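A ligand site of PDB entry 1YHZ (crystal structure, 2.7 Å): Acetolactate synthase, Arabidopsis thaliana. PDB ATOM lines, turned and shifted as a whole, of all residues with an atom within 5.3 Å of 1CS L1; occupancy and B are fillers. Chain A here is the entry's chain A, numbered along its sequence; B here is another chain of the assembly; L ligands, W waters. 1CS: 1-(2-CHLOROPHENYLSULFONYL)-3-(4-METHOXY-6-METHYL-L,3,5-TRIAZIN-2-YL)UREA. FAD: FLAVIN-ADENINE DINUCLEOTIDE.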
ATOM      1  N   MET A 266     -20.512 -12.407  10.117  1.00  0.00           N
ATOM      2  CA  MET A 266     -21.277 -12.869  11.270  1.00  0.00           C
ATOM      3  C   MET A 266     -21.907 -14.240  11.058  1.00  0.00           C
ATOM      4  O   MET A 266     -21.817 -15.116  11.926  1.00  0.00           O
ATOM      5  CB  MET A 266     -22.354 -11.840  11.612  1.00  0.00           C
ATOM      6  CG  MET A 266     -23.283 -12.258  12.729  1.00  0.00           C
ATOM      7  SD  MET A 266     -24.282 -10.892  13.355  1.00  0.00           S
ATOM      8  CE  MET A 266     -23.122 -10.175  14.541  1.00  0.00           C
ATOM      9  N   HIS A 267     -22.549 -14.421   9.913  1.00  0.00           N
ATOM     10  CA  HIS A 267     -23.190 -15.685   9.587  1.00  0.00           C
ATOM     11  C   HIS A 267     -22.566 -16.306   8.355  1.00  0.00           C
ATOM     12  O   HIS A 267     -23.239 -17.002   7.586  1.00  0.00           O
ATOM     13  CB  HIS A 267     -24.677 -15.488   9.373  1.00  0.00           C
ATOM     14  CG  HIS A 267     -25.424 -15.153  10.627  1.00  0.00           C
ATOM     15  ND1 HIS A 267     -25.476 -15.990  11.712  1.00  0.00           N
ATOM     16  CD2 HIS A 267     -26.169 -14.069  10.961  1.00  0.00           C
ATOM     17  CE1 HIS A 267     -26.214 -15.450  12.661  1.00  0.00           C
ATOM     18  NE2 HIS A 267     -26.648 -14.273  12.232  1.00  0.00           N
ATOM     19  N   ASP A 291     -19.082  -3.826  10.034  1.00  0.00           N
ATOM     20  CA  ASP A 291     -18.924  -4.506  11.319  1.00  0.00           C
ATOM     21  C   ASP A 291     -19.511  -5.908  11.291  1.00  0.00           C
ATOM     22  O   ASP A 291     -19.089  -6.781  12.044  1.00  0.00           O
ATOM     23  CB  ASP A 291     -19.568  -3.705  12.467  1.00  0.00           C
ATOM     24  CG  ASP A 291     -21.080  -3.582  12.344  1.00  0.00           C
ATOM     25  OD1 ASP A 291     -21.565  -2.621  11.699  1.00  0.00           O
ATOM     26  OD2 ASP A 291     -21.774  -4.460  12.887  1.00  0.00           O
ATOM     27  N   ARG A 292     -20.476  -6.132  10.404  1.00  0.00           N
ATOM     28  CA  ARG A 292     -21.093  -7.443  10.245  1.00  0.00           C
ATOM     29  C   ARG A 292     -20.137  -8.469   9.673  1.00  0.00           C
ATOM     30  O   ARG A 292     -20.275  -9.670   9.896  1.00  0.00           O
ATOM     31  CB  ARG A 292     -22.305  -7.340   9.318  1.00  0.00           C
ATOM     32  CG  ARG A 292     -23.627  -7.395  10.027  1.00  0.00           C
ATOM     33  CD  ARG A 292     -23.566  -6.599  11.301  1.00  0.00           C
ATOM     34  NE  ARG A 292     -24.338  -7.268  12.336  1.00  0.00           N
ATOM     35  CZ  ARG A 292     -24.407  -6.865  13.597  1.00  0.00           C
ATOM     36  NH1 ARG A 292     -23.747  -5.787  14.014  1.00  0.00           N
ATOM     37  NH2 ARG A 292     -25.161  -7.546  14.455  1.00  0.00           N
ATOM     38  N   MET A 485     -34.746 -13.746  13.998  1.00  0.00           N
ATOM     39  CA  MET A 485     -33.438 -13.267  14.438  1.00  0.00           C
ATOM     40  C   MET A 485     -33.424 -12.698  15.857  1.00  0.00           C
ATOM     41  O   MET A 485     -32.477 -12.940  16.610  1.00  0.00           O
ATOM     42  CB  MET A 485     -32.890 -12.239  13.462  1.00  0.00           C
ATOM     43  CG  MET A 485     -31.419 -11.926  13.691  1.00  0.00           C
ATOM     44  SD  MET A 485     -30.367 -13.391  13.567  1.00  0.00           S
ATOM     45  CE  MET A 485     -30.338 -13.609  11.800  1.00  0.00           C
ATOM     46  N   VAL A 486     -34.469 -11.963  16.232  1.00  0.00           N
ATOM     47  CA  VAL A 486     -34.512 -11.416  17.578  1.00  0.00           C
ATOM     48  C   VAL A 486     -34.683 -12.560  18.564  1.00  0.00           C
ATOM     49  O   VAL A 486     -34.089 -12.576  19.641  1.00  0.00           O
ATOM     50  CB  VAL A 486     -35.651 -10.426  17.765  1.00  0.00           C
ATOM     51  CG1 VAL A 486     -35.562  -9.802  19.158  1.00  0.00           C
ATOM     52  CG2 VAL A 486     -35.574  -9.348  16.699  1.00  0.00           C
ATOM     53  N   TRP A 489     -31.461 -14.327  19.260  1.00  0.00           N
ATOM     54  CA  TRP A 489     -30.651 -13.584  20.198  1.00  0.00           C
ATOM     55  C   TRP A 489     -31.195 -13.720  21.613  1.00  0.00           C
ATOM     56  O   TRP A 489     -30.435 -13.696  22.585  1.00  0.00           O
ATOM     57  CB  TRP A 489     -30.559 -12.113  19.774  1.00  0.00           C
ATOM     58  CG  TRP A 489     -29.511 -11.890  18.716  1.00  0.00           C
ATOM     59  CD1 TRP A 489     -29.433 -12.498  17.489  1.00  0.00           C
ATOM     60  CD2 TRP A 489     -28.357 -11.046  18.816  1.00  0.00           C
ATOM     61  NE1 TRP A 489     -28.303 -12.084  16.821  1.00  0.00           N
ATOM     62  CE2 TRP A 489     -27.626 -11.193  17.618  1.00  0.00           C
ATOM     63  CE3 TRP A 489     -27.870 -10.182  19.803  1.00  0.00           C
ATOM     64  CZ2 TRP A 489     -26.425 -10.503  17.381  1.00  0.00           C
ATOM     65  CZ3 TRP A 489     -26.685  -9.497  19.570  1.00  0.00           C
ATOM     66  CH2 TRP A 489     -25.970  -9.667  18.375  1.00  0.00           C
ATOM     67  N   SER A 568     -21.647 -10.208  17.699  1.00  0.00           N
ATOM     68  CA  SER A 568     -21.224  -8.855  17.349  1.00  0.00           C
ATOM     69  C   SER A 568     -19.964  -8.396  18.062  1.00  0.00           C
ATOM     70  O   SER A 568     -19.864  -8.468  19.286  1.00  0.00           O
ATOM     71  CB  SER A 568     -22.357  -7.872  17.638  1.00  0.00           C
ATOM     72  OG  SER A 568     -22.002  -6.559  17.225  1.00  0.00           O
ATOM     73  N   GLY B  35     -36.313  -4.884  18.051  1.00  0.00           N
ATOM     74  CA  GLY B  35     -35.262  -4.902  17.048  1.00  0.00           C
ATOM     75  C   GLY B  35     -33.947  -5.017  17.810  1.00  0.00           C
ATOM     76  O   GLY B  35     -33.904  -4.783  19.016  1.00  0.00           O
ATOM     77  N   GLY B  36     -32.869  -5.374  17.105  1.00  0.00           N
ATOM     78  CA  GLY B  36     -31.581  -5.520  17.754  1.00  0.00           C
ATOM     79  C   GLY B  36     -31.150  -4.394  18.675  1.00  0.00           C
ATOM     80  O   GLY B  36     -30.807  -4.618  19.842  1.00  0.00           O
ATOM     81  N   ALA B  37     -31.147  -3.163  18.162  1.00  0.00           N
ATOM     82  CA  ALA B  37     -30.733  -2.010  18.942  1.00  0.00           C
ATOM     83  C   ALA B  37     -31.636  -1.710  20.137  1.00  0.00           C
ATOM     84  O   ALA B  37     -31.241  -0.975  21.045  1.00  0.00           O
ATOM     85  CB  ALA B  37     -30.614  -0.788  18.044  1.00  0.00           C
ATOM     86  N   MET B  39     -33.404  -4.342  21.892  1.00  0.00           N
ATOM     87  CA  MET B  39     -33.672  -5.566  22.642  1.00  0.00           C
ATOM     88  C   MET B  39     -33.627  -5.352  24.150  1.00  0.00           C
ATOM     89  O   MET B  39     -34.535  -5.773  24.860  1.00  0.00           O
ATOM     90  CB  MET B  39     -32.680  -6.659  22.277  1.00  0.00           C
ATOM     91  CG  MET B  39     -32.948  -7.326  20.957  1.00  0.00           C
ATOM     92  SD  MET B  39     -31.990  -8.824  20.793  1.00  0.00           S
ATOM     93  CE  MET B  39     -32.987  -9.965  21.763  1.00  0.00           C
ATOM     94  N   SER B  83     -33.265   0.659  15.977  1.00  0.00           N
ATOM     95  CA  SER B  83     -32.524   1.593  15.151  1.00  0.00           C
ATOM     96  C   SER B  83     -32.809   1.453  13.662  1.00  0.00           C
ATOM     97  O   SER B  83     -33.517   0.534  13.243  1.00  0.00           O
ATOM     98  CB  SER B  83     -31.014   1.428  15.397  1.00  0.00           C
ATOM     99  OG  SER B  83     -30.586   0.114  15.090  1.00  0.00           O
ATOM    100  N   GLN B 110     -30.377   2.929  19.256  1.00  0.00           N
ATOM    101  CA  GLN B 110     -29.333   3.397  18.345  1.00  0.00           C
ATOM    102  C   GLN B 110     -28.197   2.418  18.456  1.00  0.00           C
ATOM    103  O   GLN B 110     -28.128   1.630  19.404  1.00  0.00           O
ATOM    104  CB  GLN B 110     -28.800   4.771  18.757  1.00  0.00           C
ATOM    105  CG  GLN B 110     -28.996   5.882  17.747  1.00  0.00           C
ATOM    106  CD  GLN B 110     -28.477   5.571  16.357  1.00  0.00           C
ATOM    107  OE1 GLN B 110     -28.641   6.373  15.446  1.00  0.00           O
ATOM    108  NE2 GLN B 110     -27.850   4.419  16.172  1.00  0.00           N
ATOM    109  N   VAL B 111     -27.289   2.484  17.496  1.00  0.00           N
ATOM    110  CA  VAL B 111     -26.113   1.637  17.501  1.00  0.00           C
ATOM    111  C   VAL B 111     -25.263   2.137  18.675  1.00  0.00           C
ATOM    112  O   VAL B 111     -25.482   3.231  19.190  1.00  0.00           O
ATOM    113  CB  VAL B 111     -25.349   1.809  16.177  1.00  0.00           C
ATOM    114  CG1 VAL B 111     -26.245   1.433  15.013  1.00  0.00           C
ATOM    115  CG2 VAL B 111     -24.893   3.246  16.025  1.00  0.00           C
ATOM    116  N   PRO B 112     -24.284   1.329  19.107  1.00  0.00           N
ATOM    117  CA  PRO B 112     -23.429   1.763  20.215  1.00  0.00           C
ATOM    118  C   PRO B 112     -22.784   3.105  19.879  1.00  0.00           C
ATOM    119  O   PRO B 112     -22.393   3.340  18.740  1.00  0.00           O
ATOM    120  CB  PRO B 112     -22.415   0.634  20.314  1.00  0.00           C
ATOM    121  CG  PRO B 112     -23.195  -0.558  19.851  1.00  0.00           C
ATOM    122  CD  PRO B 112     -23.916  -0.018  18.637  1.00  0.00           C
ATOM    123  N   MET B 115     -19.850   3.720  17.514  1.00  0.00           N
ATOM    124  CA  MET B 115     -20.076   3.398  16.105  1.00  0.00           C
ATOM    125  C   MET B 115     -20.923   4.410  15.374  1.00  0.00           C
ATOM    126  O   MET B 115     -21.117   4.306  14.165  1.00  0.00           O
ATOM    127  CB  MET B 115     -20.703   2.015  16.002  1.00  0.00           C
ATOM    128  CG  MET B 115     -19.880   0.971  16.700  1.00  0.00           C
ATOM    129  SD  MET B 115     -20.486  -0.668  16.408  1.00  0.00           S
ATOM    130  CE  MET B 115     -19.679  -1.043  14.821  1.00  0.00           C
ATOM    131  N   ALA B 120     -22.720   2.095  10.500  1.00  0.00           N
ATOM    132  CA  ALA B 120     -22.843   0.807  11.170  1.00  0.00           C
ATOM    133  C   ALA B 120     -24.120   0.091  10.784  1.00  0.00           C
ATOM    134  O   ALA B 120     -25.008   0.641  10.142  1.00  0.00           O
ATOM    135  CB  ALA B 120     -22.798   1.021  12.678  1.00  0.00           C
ATOM    136  N   PHE B 121     -24.197  -1.172  11.198  1.00  0.00           N
ATOM    137  CA  PHE B 121     -25.352  -2.012  10.943  1.00  0.00           C
ATOM    138  C   PHE B 121     -26.625  -1.338  11.443  1.00  0.00           C
ATOM    139  O   PHE B 121     -26.713  -0.928  12.599  1.00  0.00           O
ATOM    140  CB  PHE B 121     -25.158  -3.352  11.647  1.00  0.00           C
ATOM    141  CG  PHE B 121     -26.295  -4.312  11.444  1.00  0.00           C
ATOM    142  CD1 PHE B 121     -26.687  -4.687  10.170  1.00  0.00           C
ATOM    143  CD2 PHE B 121     -26.946  -4.875  12.546  1.00  0.00           C
ATOM    144  CE1 PHE B 121     -27.724  -5.596   9.984  1.00  0.00           C
ATOM    145  CE2 PHE B 121     -27.977  -5.795  12.366  1.00  0.00           C
ATOM    146  CZ  PHE B 121     -28.365  -6.158  11.077  1.00  0.00           C
ATOM    147  N   LYS B 171     -27.343   1.540  22.137  1.00  0.00           N
ATOM    148  CA  LYS B 171     -27.380   0.238  22.781  1.00  0.00           C
ATOM    149  C   LYS B 171     -26.420   0.062  23.935  1.00  0.00           C
ATOM    150  O   LYS B 171     -26.770  -0.549  24.950  1.00  0.00           O
ATOM    151  CB  LYS B 171     -27.137  -0.871  21.745  1.00  0.00           C
ATOM    152  CG  LYS B 171     -27.170  -2.284  22.312  1.00  0.00           C
ATOM    153  CD  LYS B 171     -27.582  -3.286  21.248  1.00  0.00           C
ATOM    154  CE  LYS B 171     -27.683  -4.706  21.790  1.00  0.00           C
ATOM    155  NZ  LYS B 171     -26.339  -5.305  22.045  1.00  0.00           N
HETATM  156  C5' 1CS L   1     -28.225 -10.059  12.738  1.00  0.00           C
HETATM  157  O4' 1CS L   1     -27.580  -9.190  13.640  1.00  0.00           O
HETATM  158  C4' 1CS L   1     -28.206  -8.813  14.883  1.00  0.00           C
HETATM  159  N5' 1CS L   1     -29.491  -9.336  15.181  1.00  0.00           N
HETATM  160  C6' 1CS L   1     -30.098  -8.943  16.442  1.00  0.00           C
HETATM  161  C7' 1CS L   1     -31.389  -9.471  16.734  1.00  0.00           C
HETATM  162  N1' 1CS L   1     -29.431  -8.065  17.345  1.00  0.00           N
HETATM  163  C2' 1CS L   1     -28.127  -7.574  16.987  1.00  0.00           C
HETATM  164  N10 1CS L   1     -27.468  -6.736  17.815  1.00  0.00           N
HETATM  165  C9  1CS L   1     -26.239  -6.209  17.571  1.00  0.00           C
HETATM  166  O9  1CS L   1     -25.499  -6.376  16.584  1.00  0.00           O
HETATM  167  N8  1CS L   1     -25.904  -5.393  18.608  1.00  0.00           N
HETATM  168  S7  1CS L   1     -24.466  -4.546  18.644  1.00  0.00           S
HETATM  169  O7A 1CS L   1     -23.213  -5.146  18.979  1.00  0.00           O
HETATM  170  O7B 1CS L   1     -25.095  -3.634  19.596  1.00  0.00           O
HETATM  171  C2  1CS L   1     -24.552  -3.467  17.242  1.00  0.00           C
HETATM  172  C3  1CS L   1     -23.237  -3.370  16.605  1.00  0.00           C
HETATM  173  C4  1CS L   1     -23.067  -2.524  15.389  1.00  0.00           C
HETATM  174  C5  1CS L   1     -24.231  -1.775  14.831  1.00  0.00           C
HETATM  175  C6  1CS L   1     -25.501  -1.879  15.461  1.00  0.00           C
HETATM  176  C1  1CS L   1     -25.695  -2.712  16.656  1.00  0.00           C
HETATM  177  N3' 1CS L   1     -27.569  -7.971  15.748  1.00  0.00           N
HETATM  178 CL11 1CS L   1     -27.254  -2.765  17.327  1.00  0.00          CL
HETATM  179  PA  FAD L   2     -21.859  -2.490  -0.031  1.00  0.00           P
HETATM  180  O1A FAD L   2     -22.728  -2.460  -1.239  1.00  0.00           O
HETATM  181  O2A FAD L   2     -22.369  -2.174   1.261  1.00  0.00           O
HETATM  182  O5B FAD L   2     -20.643  -1.615  -0.192  1.00  0.00           O
HETATM  183  C5B FAD L   2     -19.948  -1.661  -1.489  1.00  0.00           C
HETATM  184  C4B FAD L   2     -18.708  -0.817  -1.445  1.00  0.00           C
HETATM  185  O4B FAD L   2     -18.186  -0.918  -2.768  1.00  0.00           O
HETATM  186  C3B FAD L   2     -18.681   0.748  -1.123  1.00  0.00           C
HETATM  187  O3B FAD L   2     -17.613   1.186  -0.310  1.00  0.00           O
HETATM  188  C2B FAD L   2     -18.776   1.326  -2.487  1.00  0.00           C
HETATM  189  O2B FAD L   2     -18.698   2.680  -2.694  1.00  0.00           O
HETATM  190  C1B FAD L   2     -17.842   0.370  -3.232  1.00  0.00           C
HETATM  191  N9A FAD L   2     -18.015   0.327  -4.769  1.00  0.00           N
HETATM  192  C8A FAD L   2     -19.329   0.513  -5.392  1.00  0.00           C
HETATM  193  N7A FAD L   2     -19.359   0.460  -6.699  1.00  0.00           N
HETATM  194  C5A FAD L   2     -18.070   0.256  -7.048  1.00  0.00           C
HETATM  195  C6A FAD L   2     -17.243   0.065  -8.360  1.00  0.00           C
HETATM  196  N6A FAD L   2     -17.835   0.098  -9.541  1.00  0.00           N
HETATM  197  N1A FAD L   2     -15.804  -0.144  -8.288  1.00  0.00           N
HETATM  198  C2A FAD L   2     -15.121  -0.194  -7.002  1.00  0.00           C
HETATM  199  N3A FAD L   2     -15.764  -0.036  -5.771  1.00  0.00           N
HETATM  200  C4A FAD L   2     -17.221   0.179  -5.830  1.00  0.00           C
HETATM  201  N1  FAD L   2     -22.976  -9.241   5.504  1.00  0.00           N
HETATM  202  C2  FAD L   2     -22.011 -10.166   5.427  1.00  0.00           C
HETATM  203  O2  FAD L   2     -21.192 -10.064   4.511  1.00  0.00           O
HETATM  204  N3  FAD L   2     -21.975 -11.267   6.308  1.00  0.00           N
HETATM  205  C4  FAD L   2     -22.984 -11.476   7.296  1.00  0.00           C
HETATM  206  O4  FAD L   2     -22.905 -12.385   8.135  1.00  0.00           O
HETATM  207  C4X FAD L   2     -24.092 -10.517   7.308  1.00  0.00           C
HETATM  208  N5  FAD L   2     -25.134 -10.700   8.189  1.00  0.00           N
HETATM  209  C5X FAD L   2     -26.186  -9.805   8.164  1.00  0.00           C
HETATM  210  C6  FAD L   2     -27.341 -10.111   8.966  1.00  0.00           C
HETATM  211  C7  FAD L   2     -28.524  -9.337   8.846  1.00  0.00           C
HETATM  212  C7M FAD L   2     -29.765  -9.802   9.573  1.00  0.00           C
HETATM  213  C8  FAD L   2     -28.544  -8.172   7.943  1.00  0.00           C
HETATM  214  C8M FAD L   2     -29.797  -7.361   7.661  1.00  0.00           C
HETATM  215  C9  FAD L   2     -27.369  -7.826   7.219  1.00  0.00           C
HETATM  216  C9A FAD L   2     -26.199  -8.646   7.258  1.00  0.00           C
HETATM  217  N10 FAD L   2     -25.042  -8.404   6.458  1.00  0.00           N
HETATM  218  C10 FAD L   2     -24.025  -9.373   6.399  1.00  0.00           C
HETATM  219  C1' FAD L   2     -25.067  -7.338   5.393  1.00  0.00           C
HETATM  220  C2' FAD L   2     -24.263  -6.254   5.974  1.00  0.00           C
HETATM  221  O2' FAD L   2     -25.028  -5.423   6.835  1.00  0.00           O
HETATM  222  C3' FAD L   2     -23.636  -5.273   4.955  1.00  0.00           C
HETATM  223  O3' FAD L   2     -24.820  -4.750   4.141  1.00  0.00           O
HETATM  224  C4' FAD L   2     -22.687  -5.907   3.883  1.00  0.00           C
HETATM  225  O4' FAD L   2     -21.610  -6.666   4.659  1.00  0.00           O
HETATM  226  C5' FAD L   2     -22.076  -4.847   3.083  1.00  0.00           C
HETATM  227  O5' FAD L   2     -21.181  -5.511   2.143  1.00  0.00           O
HETATM  228  P   FAD L   2     -20.349  -4.728   1.099  1.00  0.00           P
HETATM  229  O1P FAD L   2     -19.503  -3.780   1.871  1.00  0.00           O
HETATM  230  O2P FAD L   2     -19.590  -5.715   0.412  1.00  0.00           O
HETATM  231  O3P FAD L   2     -21.300  -4.004   0.052  1.00  0.00           O
HETATM  232  O   HOH W   1     -27.062 -12.450  14.517  1.00  0.00           O
HETATM  233  O   HOH W   2     -29.142  -6.789  20.092  1.00  0.00           O
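The backbone NH (N) of His 267 is in hydrogen-bond range of an oxygen (O4) of FAD L2 (2.7 Å).
O7A of 1CS L1 is in hydrogen-bond range of OG of Ser 568.
The indole nitrogen (NE1) of Trp 489 is in hydrogen-bond range of a nitrogen (N5') of 1CS L1, at 3.4 Å.
NH2 of Arg 292 lies within hydrogen-bond range of O9 of 1CS L1 (2.5 Å).
NZ of Lys 171 of chain B lies close to O7B of 1CS L1 (3.2 Å).
The backbone NH of Met 266 is in hydrogen-bond range of an oxygen (O4) of FAD L2 (3.1 Å).
OD1 of Asp 291 sits at hydrogen-bond distance from N of Phe 121 of chain B, 3.0 Å away.
The guanidinium group (NH1) of Arg 292 is in salt-bridge range of the side-chain carboxylate (OD2) of Asp 291 (2.6 Å).
O of Arg 292 is in hydrogen-bond range of N of Met 266, at 2.8 Å.
An oxygen (O4') of 1CS L1 sits close to the side-chain sulfur of Met 266, at 3.7 Å.
Asp 291 touches 1CS L1 (OD2 to C4, 3.4 Å).
Met 485 touches 1CS L1 (CG to N5', 3.6 Å).
Val 486 touches 1CS L1.
Gly 36 of chain B touches 1CS L1.
Ala 37 of chain B touches 1CS L1.
Val 111 of chain B touches 1CS L1.
CG of Pro 112 of chain B touches O7B of 1CS L1, 3.6 Å away.
SD of Met 115 of chain B touches C4 of 1CS L1 (3.3 Å).
Ala 120 of chain B touches 1CS L1.
Phe 121 of chain B touches 1CS L1.
Hydrophobic or aromatic side chains that line 1CS L1: Met 266, Met 485, Trp 489, Ala 37 of chain B, Val 111 of chain B, Pro 112 of chain B, Met 115 of chain B, Ala 120 of chain B and Phe 121 of chain B.
Within 4 Å of 1CS L1: Met 266, Asp 291, Arg 292, Met 485, Val 486, Trp 489, Ser 568, Gly 36 of chain B, Ala 37 of chain B, Val 111 of chain B, Pro 112 of chain B, Met 115 of chain B, Ala 120 of chain B, Phe 121 of chain B and Lys 171 of chain B.
The nearest printed residue that does not touch 1CS L1 is Met 39 of chain B (4.2 Å).
Water W2 lies within hydrogen-bond range of the backbone carbonyl oxygen (O) of Gly 36 of chain B (2.7 Å), a nitrogen (N10) of 1CS L1 (2.8 Å) and the side-chain sulfur (SD) of Met 39 of chain B (3.6 Å).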
